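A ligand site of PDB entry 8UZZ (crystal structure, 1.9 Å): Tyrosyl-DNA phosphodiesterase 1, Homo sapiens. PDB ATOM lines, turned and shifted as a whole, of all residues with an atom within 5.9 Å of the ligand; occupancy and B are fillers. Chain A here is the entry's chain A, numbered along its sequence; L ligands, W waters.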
ATOM      1  N   ASN A  56      17.616 -13.828   4.972  1.00  0.00           N
ATOM      2  CA  ASN A  56      16.746 -14.418   3.962  1.00  0.00           C
ATOM      3  C   ASN A  56      16.146 -13.348   3.063  1.00  0.00           C
ATOM      4  O   ASN A  56      16.465 -12.164   3.152  1.00  0.00           O
ATOM      5  CB  ASN A  56      15.645 -15.263   4.616  1.00  0.00           C
ATOM      6  CG  ASN A  56      15.393 -16.557   3.842  1.00  0.00           C
ATOM      7  OD1 ASN A  56      14.815 -16.522   2.756  1.00  0.00           O
ATOM      8  ND2 ASN A  56      15.850 -17.669   4.362  1.00  0.00           N
ATOM      9  N   TYR A  57      15.280 -13.805   2.160  1.00  0.00           N
ATOM     10  CA  TYR A  57      14.542 -12.938   1.260  1.00  0.00           C
ATOM     11  C   TYR A  57      13.105 -12.766   1.724  1.00  0.00           C
ATOM     12  O   TYR A  57      12.659 -11.644   1.998  1.00  0.00           O
ATOM     13  CB  TYR A  57      14.618 -13.514  -0.165  1.00  0.00           C
ATOM     14  CG  TYR A  57      13.718 -12.797  -1.126  1.00  0.00           C
ATOM     15  CD1 TYR A  57      13.851 -11.422  -1.333  1.00  0.00           C
ATOM     16  CD2 TYR A  57      12.697 -13.454  -1.794  1.00  0.00           C
ATOM     17  CE1 TYR A  57      13.004 -10.730  -2.204  1.00  0.00           C
ATOM     18  CE2 TYR A  57      11.851 -12.770  -2.671  1.00  0.00           C
ATOM     19  CZ  TYR A  57      12.015 -11.414  -2.868  1.00  0.00           C
ATOM     20  OH  TYR A  57      11.179 -10.735  -3.737  1.00  0.00           O
ATOM     21  N   CYS A  58      12.364 -13.872   1.839  1.00  0.00           N
ATOM     22  CA  CYS A  58      10.965 -13.844   2.248  1.00  0.00           C
ATOM     23  C   CYS A  58      10.796 -14.528   3.602  1.00  0.00           C
ATOM     24  O   CYS A  58      11.376 -15.585   3.847  1.00  0.00           O
ATOM     25  CB  CYS A  58      10.091 -14.532   1.205  1.00  0.00           C
ATOM     26  SG  CYS A  58       8.371 -14.338   1.566  1.00  0.00           S
ATOM     27  N   THR A 114      18.511  -7.401  -4.957  1.00  0.00           N
ATOM     28  CA  THR A 114      17.705  -8.068  -3.947  1.00  0.00           C
ATOM     29  C   THR A 114      18.620  -8.684  -2.902  1.00  0.00           C
ATOM     30  O   THR A 114      19.777  -8.993  -3.178  1.00  0.00           O
ATOM     31  CB  THR A 114      16.821  -9.157  -4.587  1.00  0.00           C
ATOM     32  OG1 THR A 114      16.191  -8.631  -5.762  1.00  0.00           O
ATOM     33  CG2 THR A 114      15.751  -9.616  -3.647  1.00  0.00           C
ATOM     34  N   HIS A 115      18.080  -8.913  -1.694  1.00  0.00           N
ATOM     35  CA  HIS A 115      18.812  -9.659  -0.670  1.00  0.00           C
ATOM     36  C   HIS A 115      18.339 -11.112  -0.721  1.00  0.00           C
ATOM     37  O   HIS A 115      17.339 -11.481  -0.090  1.00  0.00           O
ATOM     38  CB  HIS A 115      18.614  -9.053   0.721  1.00  0.00           C
ATOM     39  CG  HIS A 115      19.431  -9.723   1.782  1.00  0.00           C
ATOM     40  ND1 HIS A 115      18.967 -10.804   2.501  1.00  0.00           N
ATOM     41  CD2 HIS A 115      20.696  -9.499   2.213  1.00  0.00           C
ATOM     42  CE1 HIS A 115      19.905 -11.201   3.345  1.00  0.00           C
ATOM     43  NE2 HIS A 115      20.968 -10.427   3.183  1.00  0.00           N
ATOM     44  N   HIS A 116      19.062 -11.952  -1.473  1.00  0.00           N
ATOM     45  CA  HIS A 116      18.674 -13.342  -1.693  1.00  0.00           C
ATOM     46  C   HIS A 116      19.409 -14.337  -0.785  1.00  0.00           C
ATOM     47  O   HIS A 116      18.991 -15.496  -0.728  1.00  0.00           O
ATOM     48  CB  HIS A 116      18.910 -13.770  -3.157  1.00  0.00           C
ATOM     49  CG  HIS A 116      17.948 -13.190  -4.138  1.00  0.00           C
ATOM     50  ND1 HIS A 116      18.336 -12.771  -5.399  1.00  0.00           N
ATOM     51  CD2 HIS A 116      16.604 -12.993  -4.079  1.00  0.00           C
ATOM     52  CE1 HIS A 116      17.287 -12.323  -6.064  1.00  0.00           C
ATOM     53  NE2 HIS A 116      16.214 -12.457  -5.285  1.00  0.00           N
ATOM     54  N   LYS A 118      20.553 -16.832   1.918  1.00  0.00           N
ATOM     55  CA  LYS A 118      19.836 -17.649   2.902  1.00  0.00           C
ATOM     56  C   LYS A 118      20.851 -18.296   3.844  1.00  0.00           C
ATOM     57  O   LYS A 118      21.556 -19.239   3.474  1.00  0.00           O
ATOM     58  CB  LYS A 118      18.956 -18.659   2.170  1.00  0.00           C
ATOM     59  CG  LYS A 118      17.953 -17.852   1.316  1.00  0.00           C
ATOM     60  CD  LYS A 118      17.078 -18.666   0.429  1.00  0.00           C
ATOM     61  CE  LYS A 118      16.042 -17.777  -0.266  1.00  0.00           C
ATOM     62  NZ  LYS A 118      16.684 -16.892  -1.283  1.00  0.00           N
ATOM     63  N   THR A 134      19.088 -22.719   0.850  1.00  0.00           N
ATOM     64  CA  THR A 134      18.435 -22.141  -0.311  1.00  0.00           C
ATOM     65  C   THR A 134      16.955 -21.822  -0.108  1.00  0.00           C
ATOM     66  O   THR A 134      16.311 -21.351  -1.050  1.00  0.00           O
ATOM     67  CB  THR A 134      18.567 -23.094  -1.516  1.00  0.00           C
ATOM     68  OG1 THR A 134      17.864 -24.316  -1.253  1.00  0.00           O
ATOM     69  CG2 THR A 134      20.025 -23.412  -1.791  1.00  0.00           C
ATOM     70  N   SER A 135      16.404 -22.032   1.091  1.00  0.00           N
ATOM     71  CA  SER A 135      14.967 -21.903   1.340  1.00  0.00           C
ATOM     72  C   SER A 135      14.594 -20.586   1.983  1.00  0.00           C
ATOM     73  O   SER A 135      15.221 -20.140   2.953  1.00  0.00           O
ATOM     74  CB  SER A 135      14.477 -23.016   2.272  1.00  0.00           C
ATOM     75  OG  SER A 135      14.840 -24.290   1.808  1.00  0.00           O
ATOM     76  N   ASN A 136      13.516 -19.970   1.477  1.00  0.00           N
ATOM     77  CA  ASN A 136      12.839 -18.892   2.175  1.00  0.00           C
ATOM     78  C   ASN A 136      12.238 -19.418   3.483  1.00  0.00           C
ATOM     79  O   ASN A 136      11.994 -20.612   3.653  1.00  0.00           O
ATOM     80  CB  ASN A 136      11.738 -18.305   1.293  1.00  0.00           C
ATOM     81  CG  ASN A 136      12.316 -17.561   0.093  1.00  0.00           C
ATOM     82  OD1 ASN A 136      12.738 -16.408   0.215  1.00  0.00           O
ATOM     83  ND2 ASN A 136      12.361 -18.223  -1.059  1.00  0.00           N
ATOM     84  N   ASP A 141       8.300 -23.340   1.232  1.00  0.00           N
ATOM     85  CA  ASP A 141       9.655 -23.639   0.767  1.00  0.00           C
ATOM     86  C   ASP A 141      10.232 -24.879   1.422  1.00  0.00           C
ATOM     87  O   ASP A 141      11.219 -25.418   0.906  1.00  0.00           O
ATOM     88  CB  ASP A 141      10.575 -22.430   0.986  1.00  0.00           C
ATOM     89  CG  ASP A 141      10.715 -21.565  -0.262  1.00  0.00           C
ATOM     90  OD1 ASP A 141       9.679 -21.333  -0.934  1.00  0.00           O
ATOM     91  OD2 ASP A 141      11.846 -21.135  -0.574  1.00  0.00           O
ATOM     92  N   GLY A 311       4.754 -20.816  -8.914  1.00  0.00           N
ATOM     93  CA  GLY A 311       4.807 -19.558  -8.191  1.00  0.00           C
ATOM     94  C   GLY A 311       6.177 -19.223  -7.650  1.00  0.00           C
ATOM     95  O   GLY A 311       6.468 -18.043  -7.402  1.00  0.00           O
ATOM     96  N   SER A 312       7.044 -20.233  -7.450  1.00  0.00           N
ATOM     97  CA  SER A 312       8.439 -20.019  -7.046  1.00  0.00           C
ATOM     98  C   SER A 312       9.434 -20.318  -8.155  1.00  0.00           C
ATOM     99  O   SER A 312      10.615 -20.556  -7.876  1.00  0.00           O
ATOM    100  CB  SER A 312       8.797 -20.831  -5.802  1.00  0.00           C
ATOM    101  OG  SER A 312       7.803 -20.731  -4.811  1.00  0.00           O
ATOM    102  N   LEU A 313       8.992 -20.275  -9.414  1.00  0.00           N
ATOM    103  CA  LEU A 313       9.857 -20.422 -10.591  1.00  0.00           C
ATOM    104  C   LEU A 313       9.589 -19.205 -11.465  1.00  0.00           C
ATOM    105  O   LEU A 313       8.928 -19.283 -12.503  1.00  0.00           O
ATOM    106  CB  LEU A 313       9.566 -21.733 -11.325  1.00  0.00           C
ATOM    107  CG  LEU A 313       9.877 -23.013 -10.548  1.00  0.00           C
ATOM    108  CD1 LEU A 313       9.124 -24.256 -11.084  1.00  0.00           C
ATOM    109  CD2 LEU A 313      11.400 -23.328 -10.480  1.00  0.00           C
ATOM    110  N   PRO A 314      10.073 -18.027 -11.046  1.00  0.00           N
ATOM    111  CA  PRO A 314       9.536 -16.747 -11.564  1.00  0.00           C
ATOM    112  C   PRO A 314      10.180 -16.283 -12.870  1.00  0.00           C
ATOM    113  O   PRO A 314      10.671 -15.165 -12.985  1.00  0.00           O
ATOM    114  CB  PRO A 314       9.823 -15.776 -10.408  1.00  0.00           C
ATOM    115  CG  PRO A 314      11.097 -16.305  -9.802  1.00  0.00           C
ATOM    116  CD  PRO A 314      11.058 -17.820  -9.959  1.00  0.00           C
ATOM    117  N   HIS A 346      14.039 -25.544  -5.758  1.00  0.00           N
ATOM    118  CA  HIS A 346      14.371 -24.191  -5.389  1.00  0.00           C
ATOM    119  C   HIS A 346      15.835 -24.110  -4.949  1.00  0.00           C
ATOM    120  O   HIS A 346      16.372 -23.006  -4.733  1.00  0.00           O
ATOM    121  CB  HIS A 346      13.425 -23.700  -4.269  1.00  0.00           C
ATOM    122  CG  HIS A 346      13.529 -22.230  -3.976  1.00  0.00           C
ATOM    123  ND1 HIS A 346      14.373 -21.721  -3.010  1.00  0.00           N
ATOM    124  CD2 HIS A 346      12.854 -21.156  -4.474  1.00  0.00           C
ATOM    125  CE1 HIS A 346      14.253 -20.412  -2.954  1.00  0.00           C
ATOM    126  NE2 HIS A 346      13.335 -20.036  -3.837  1.00  0.00           N
ATOM    127  N   LYS A 348      19.775 -24.190  -5.912  1.00  0.00           N
ATOM    128  CA  LYS A 348      20.579 -23.851  -7.082  1.00  0.00           C
ATOM    129  C   LYS A 348      21.944 -24.502  -6.900  1.00  0.00           C
ATOM    130  O   LYS A 348      22.518 -24.464  -5.812  1.00  0.00           O
ATOM    131  CB  LYS A 348      20.764 -22.340  -7.269  1.00  0.00           C
ATOM    132  CG  LYS A 348      19.442 -21.589  -7.467  1.00  0.00           C
ATOM    133  CD  LYS A 348      18.837 -21.215  -6.107  1.00  0.00           C
ATOM    134  CE  LYS A 348      17.729 -20.190  -6.295  1.00  0.00           C
ATOM    135  NZ  LYS A 348      16.528 -20.518  -5.512  1.00  0.00           N
ATOM    136  N   SER A 367      22.467 -19.637  -3.272  1.00  0.00           N
ATOM    137  CA  SER A 367      21.209 -18.962  -3.566  1.00  0.00           C
ATOM    138  C   SER A 367      21.163 -18.384  -4.959  1.00  0.00           C
ATOM    139  O   SER A 367      20.092 -18.012  -5.418  1.00  0.00           O
ATOM    140  CB  SER A 367      21.008 -17.767  -2.602  1.00  0.00           C
ATOM    141  OG  SER A 367      22.135 -16.883  -2.689  1.00  0.00           O
ATOM    142  N   ASN A 369      20.733 -17.606  -8.634  1.00  0.00           N
ATOM    143  CA  ASN A 369      20.114 -18.084  -9.850  1.00  0.00           C
ATOM    144  C   ASN A 369      20.954 -17.699 -11.064  1.00  0.00           C
ATOM    145  O   ASN A 369      22.031 -17.095 -10.953  1.00  0.00           O
ATOM    146  CB  ASN A 369      18.676 -17.550  -9.976  1.00  0.00           C
ATOM    147  CG  ASN A 369      17.688 -18.407  -9.214  1.00  0.00           C
ATOM    148  OD1 ASN A 369      17.671 -19.637  -9.353  1.00  0.00           O
ATOM    149  ND2 ASN A 369      16.868 -17.765  -8.363  1.00  0.00           N
ATOM    150  N   TRP A 443       6.065 -18.264 -15.607  1.00  0.00           N
ATOM    151  CA  TRP A 443       5.065 -18.216 -14.543  1.00  0.00           C
ATOM    152  C   TRP A 443       3.901 -17.270 -14.796  1.00  0.00           C
ATOM    153  O   TRP A 443       2.866 -17.389 -14.120  1.00  0.00           O
ATOM    154  CB  TRP A 443       5.724 -17.865 -13.199  1.00  0.00           C
ATOM    155  CG  TRP A 443       6.119 -16.424 -13.017  1.00  0.00           C
ATOM    156  CD1 TRP A 443       6.439 -15.509 -13.994  1.00  0.00           C
ATOM    157  CD2 TRP A 443       6.264 -15.734 -11.770  1.00  0.00           C
ATOM    158  NE1 TRP A 443       6.753 -14.297 -13.429  1.00  0.00           N
ATOM    159  CE2 TRP A 443       6.649 -14.408 -12.063  1.00  0.00           C
ATOM    160  CE3 TRP A 443       6.085 -16.104 -10.425  1.00  0.00           C
ATOM    161  CZ2 TRP A 443       6.875 -13.460 -11.067  1.00  0.00           C
ATOM    162  CZ3 TRP A 443       6.301 -15.151  -9.437  1.00  0.00           C
ATOM    163  CH2 TRP A 443       6.697 -13.845  -9.770  1.00  0.00           C
HETATM  164  C1  LIG L   1      11.069 -12.473  -8.466  1.00  0.00           C
HETATM  165  C2  LIG L   1      10.352 -10.252  -6.961  1.00  0.00           C
HETATM  166  C3  LIG L   1       9.016 -14.734  -6.972  1.00  0.00           C
HETATM  167  C4  LIG L   1       8.822 -16.028  -6.470  1.00  0.00           C
HETATM  168  C5  LIG L   1       9.813 -16.644  -5.712  1.00  0.00           C
HETATM  169  C6  LIG L   1      12.079 -16.594  -4.640  1.00  0.00           C
HETATM  170  C7  LIG L   1      14.477 -16.391  -3.565  1.00  0.00           C
HETATM  171  C8  LIG L   1      13.297 -15.818  -4.415  1.00  0.00           C
HETATM  172  C9  LIG L   1      13.404 -14.590  -4.934  1.00  0.00           C
HETATM  173  C10 LIG L   1      11.200 -14.663  -5.953  1.00  0.00           C
HETATM  174  C11 LIG L   1      10.199 -14.036  -6.727  1.00  0.00           C
HETATM  175  C12 LIG L   1      10.449 -12.687  -7.217  1.00  0.00           C
HETATM  176  C13 LIG L   1      11.314 -11.196  -8.958  1.00  0.00           C
HETATM  177  C14 LIG L   1      10.946 -10.080  -8.189  1.00  0.00           C
HETATM  178  C15 LIG L   1      10.099 -11.552  -6.472  1.00  0.00           C
HETATM  179  C16 LIG L   1      11.017 -15.970  -5.449  1.00  0.00           C
HETATM  180  N1  LIG L   1      12.386 -14.004  -5.687  1.00  0.00           N
HETATM  181  O1  LIG L   1      14.269 -17.418  -2.920  1.00  0.00           O
HETATM  182  O2  LIG L   1      15.518 -15.736  -3.613  1.00  0.00           O
HETATM  183  O3  LIG L   1       9.483 -11.679  -5.223  1.00  0.00           O
HETATM  184  O4  LIG L   1       9.044 -11.481  -2.817  1.00  0.00           O
HETATM  185  O5  LIG L   1       9.603  -9.451  -4.045  1.00  0.00           O
HETATM  186  O6  LIG L   1      11.895 -17.734  -4.213  1.00  0.00           O
HETATM  187  S1  LIG L   1       9.720 -10.828  -3.867  1.00  0.00           S
HETATM  188  O   HOH W   1      14.376 -14.730  -8.413  1.00  0.00           O
HETATM  189  O   HOH W   2      13.446  -9.094  -6.326  1.00  0.00           O
HETATM  190  O   HOH W   3       9.700 -19.540  -2.952  1.00  0.00           O
HETATM  191  O   HOH W   4      15.032 -18.337  -6.118  1.00  0.00           O
HETATM  192  O   HOH W   5      17.671 -17.642  -4.201  1.00  0.00           O
HETATM  193  O   HOH W   6      13.831 -11.789  -6.490  1.00  0.00           O
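A ring nitrogen (NE2) of His 346 sits at hydrogen-bond distance from the side-chain amide nitrogen (ND2) of Asn 136 (3.5 Å). ND1 of His 346 is in hydrogen-bond range of O of Thr 134. The side-chain amide oxygen (OD1) of Asn 136 lies within hydrogen-bond range of the backbone NH (N) of Cys 58 (3.0 Å). The backbone carbonyl oxygen (O) of His 346 sits at hydrogen-bond distance from the side-chain amino group (NZ) of Lys 348 (2.6 Å). NZ of Lys 118 lies within hydrogen-bond range of O of His 116, at 2.8 Å. The side-chain carboxylate (OD2) of Asp 141 sits at hydrogen-bond distance from the backbone NH (N) of Asn 136 (2.9 Å). The side-chain amide oxygen (OD1) of Asn 56 sits close to the side-chain amide oxygen (OD1) of Asn 136.
O2 of the ligand lies within salt-bridge range of NZ of Lys 118 (2.9 Å). The side-chain amide nitrogen (ND2) of Asn 136 is in hydrogen-bond range of an oxygen (O1) of the ligand (2.8 Å). O6 of the ligand lies within hydrogen-bond range of NE2 of His 346 (2.7 Å). The side-chain hydroxyl (OH) of Tyr 57 is bonded to a sulfur (S1) of the ligand, at 1.5 Å.
CD2 of His 116 touches O2 of the ligand, at 3.0 Å. Gly 311 touches the ligand (O to C4, 3.2 Å). CA of Ser 312 touches C5 of the ligand, at 3.9 Å. Pro 314 touches the ligand. Trp 443 touches the ligand (CZ3 to C3, 3.7 Å). The nearest printed residue that does not touch the ligand is Lys 348 (4.6 Å).
Water W6 lies within hydrogen-bond range of a ring nitrogen (NE2) of His 116 and a nitrogen (N1) of the ligand. Water W5 lies within hydrogen-bond range of the backbone carbonyl oxygen of Ser 367 (2.7 Å), an oxygen (O2) of the ligand (2.9 Å), the side-chain amino group of Lys 118 (3.2 Å) and the side-chain amino group of Lys 348 (3.4 Å). Water W3 lies within hydrogen-bond range of the side-chain carboxylate of Asp 141 (2.7 Å), the side-chain hydroxyl of Ser 312 (2.9 Å) and an oxygen (O6) of the ligand (3.1 Å). Water W4 lies within hydrogen-bond range of the side-chain amino group (NZ) of Lys 348 (2.7 Å), the side-chain amide nitrogen (ND2) of Asn 369 (3.0 Å), a ring nitrogen (NE2) of His 346 (3.3 Å) and an oxygen (O1) of the ligand (3.4 Å).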
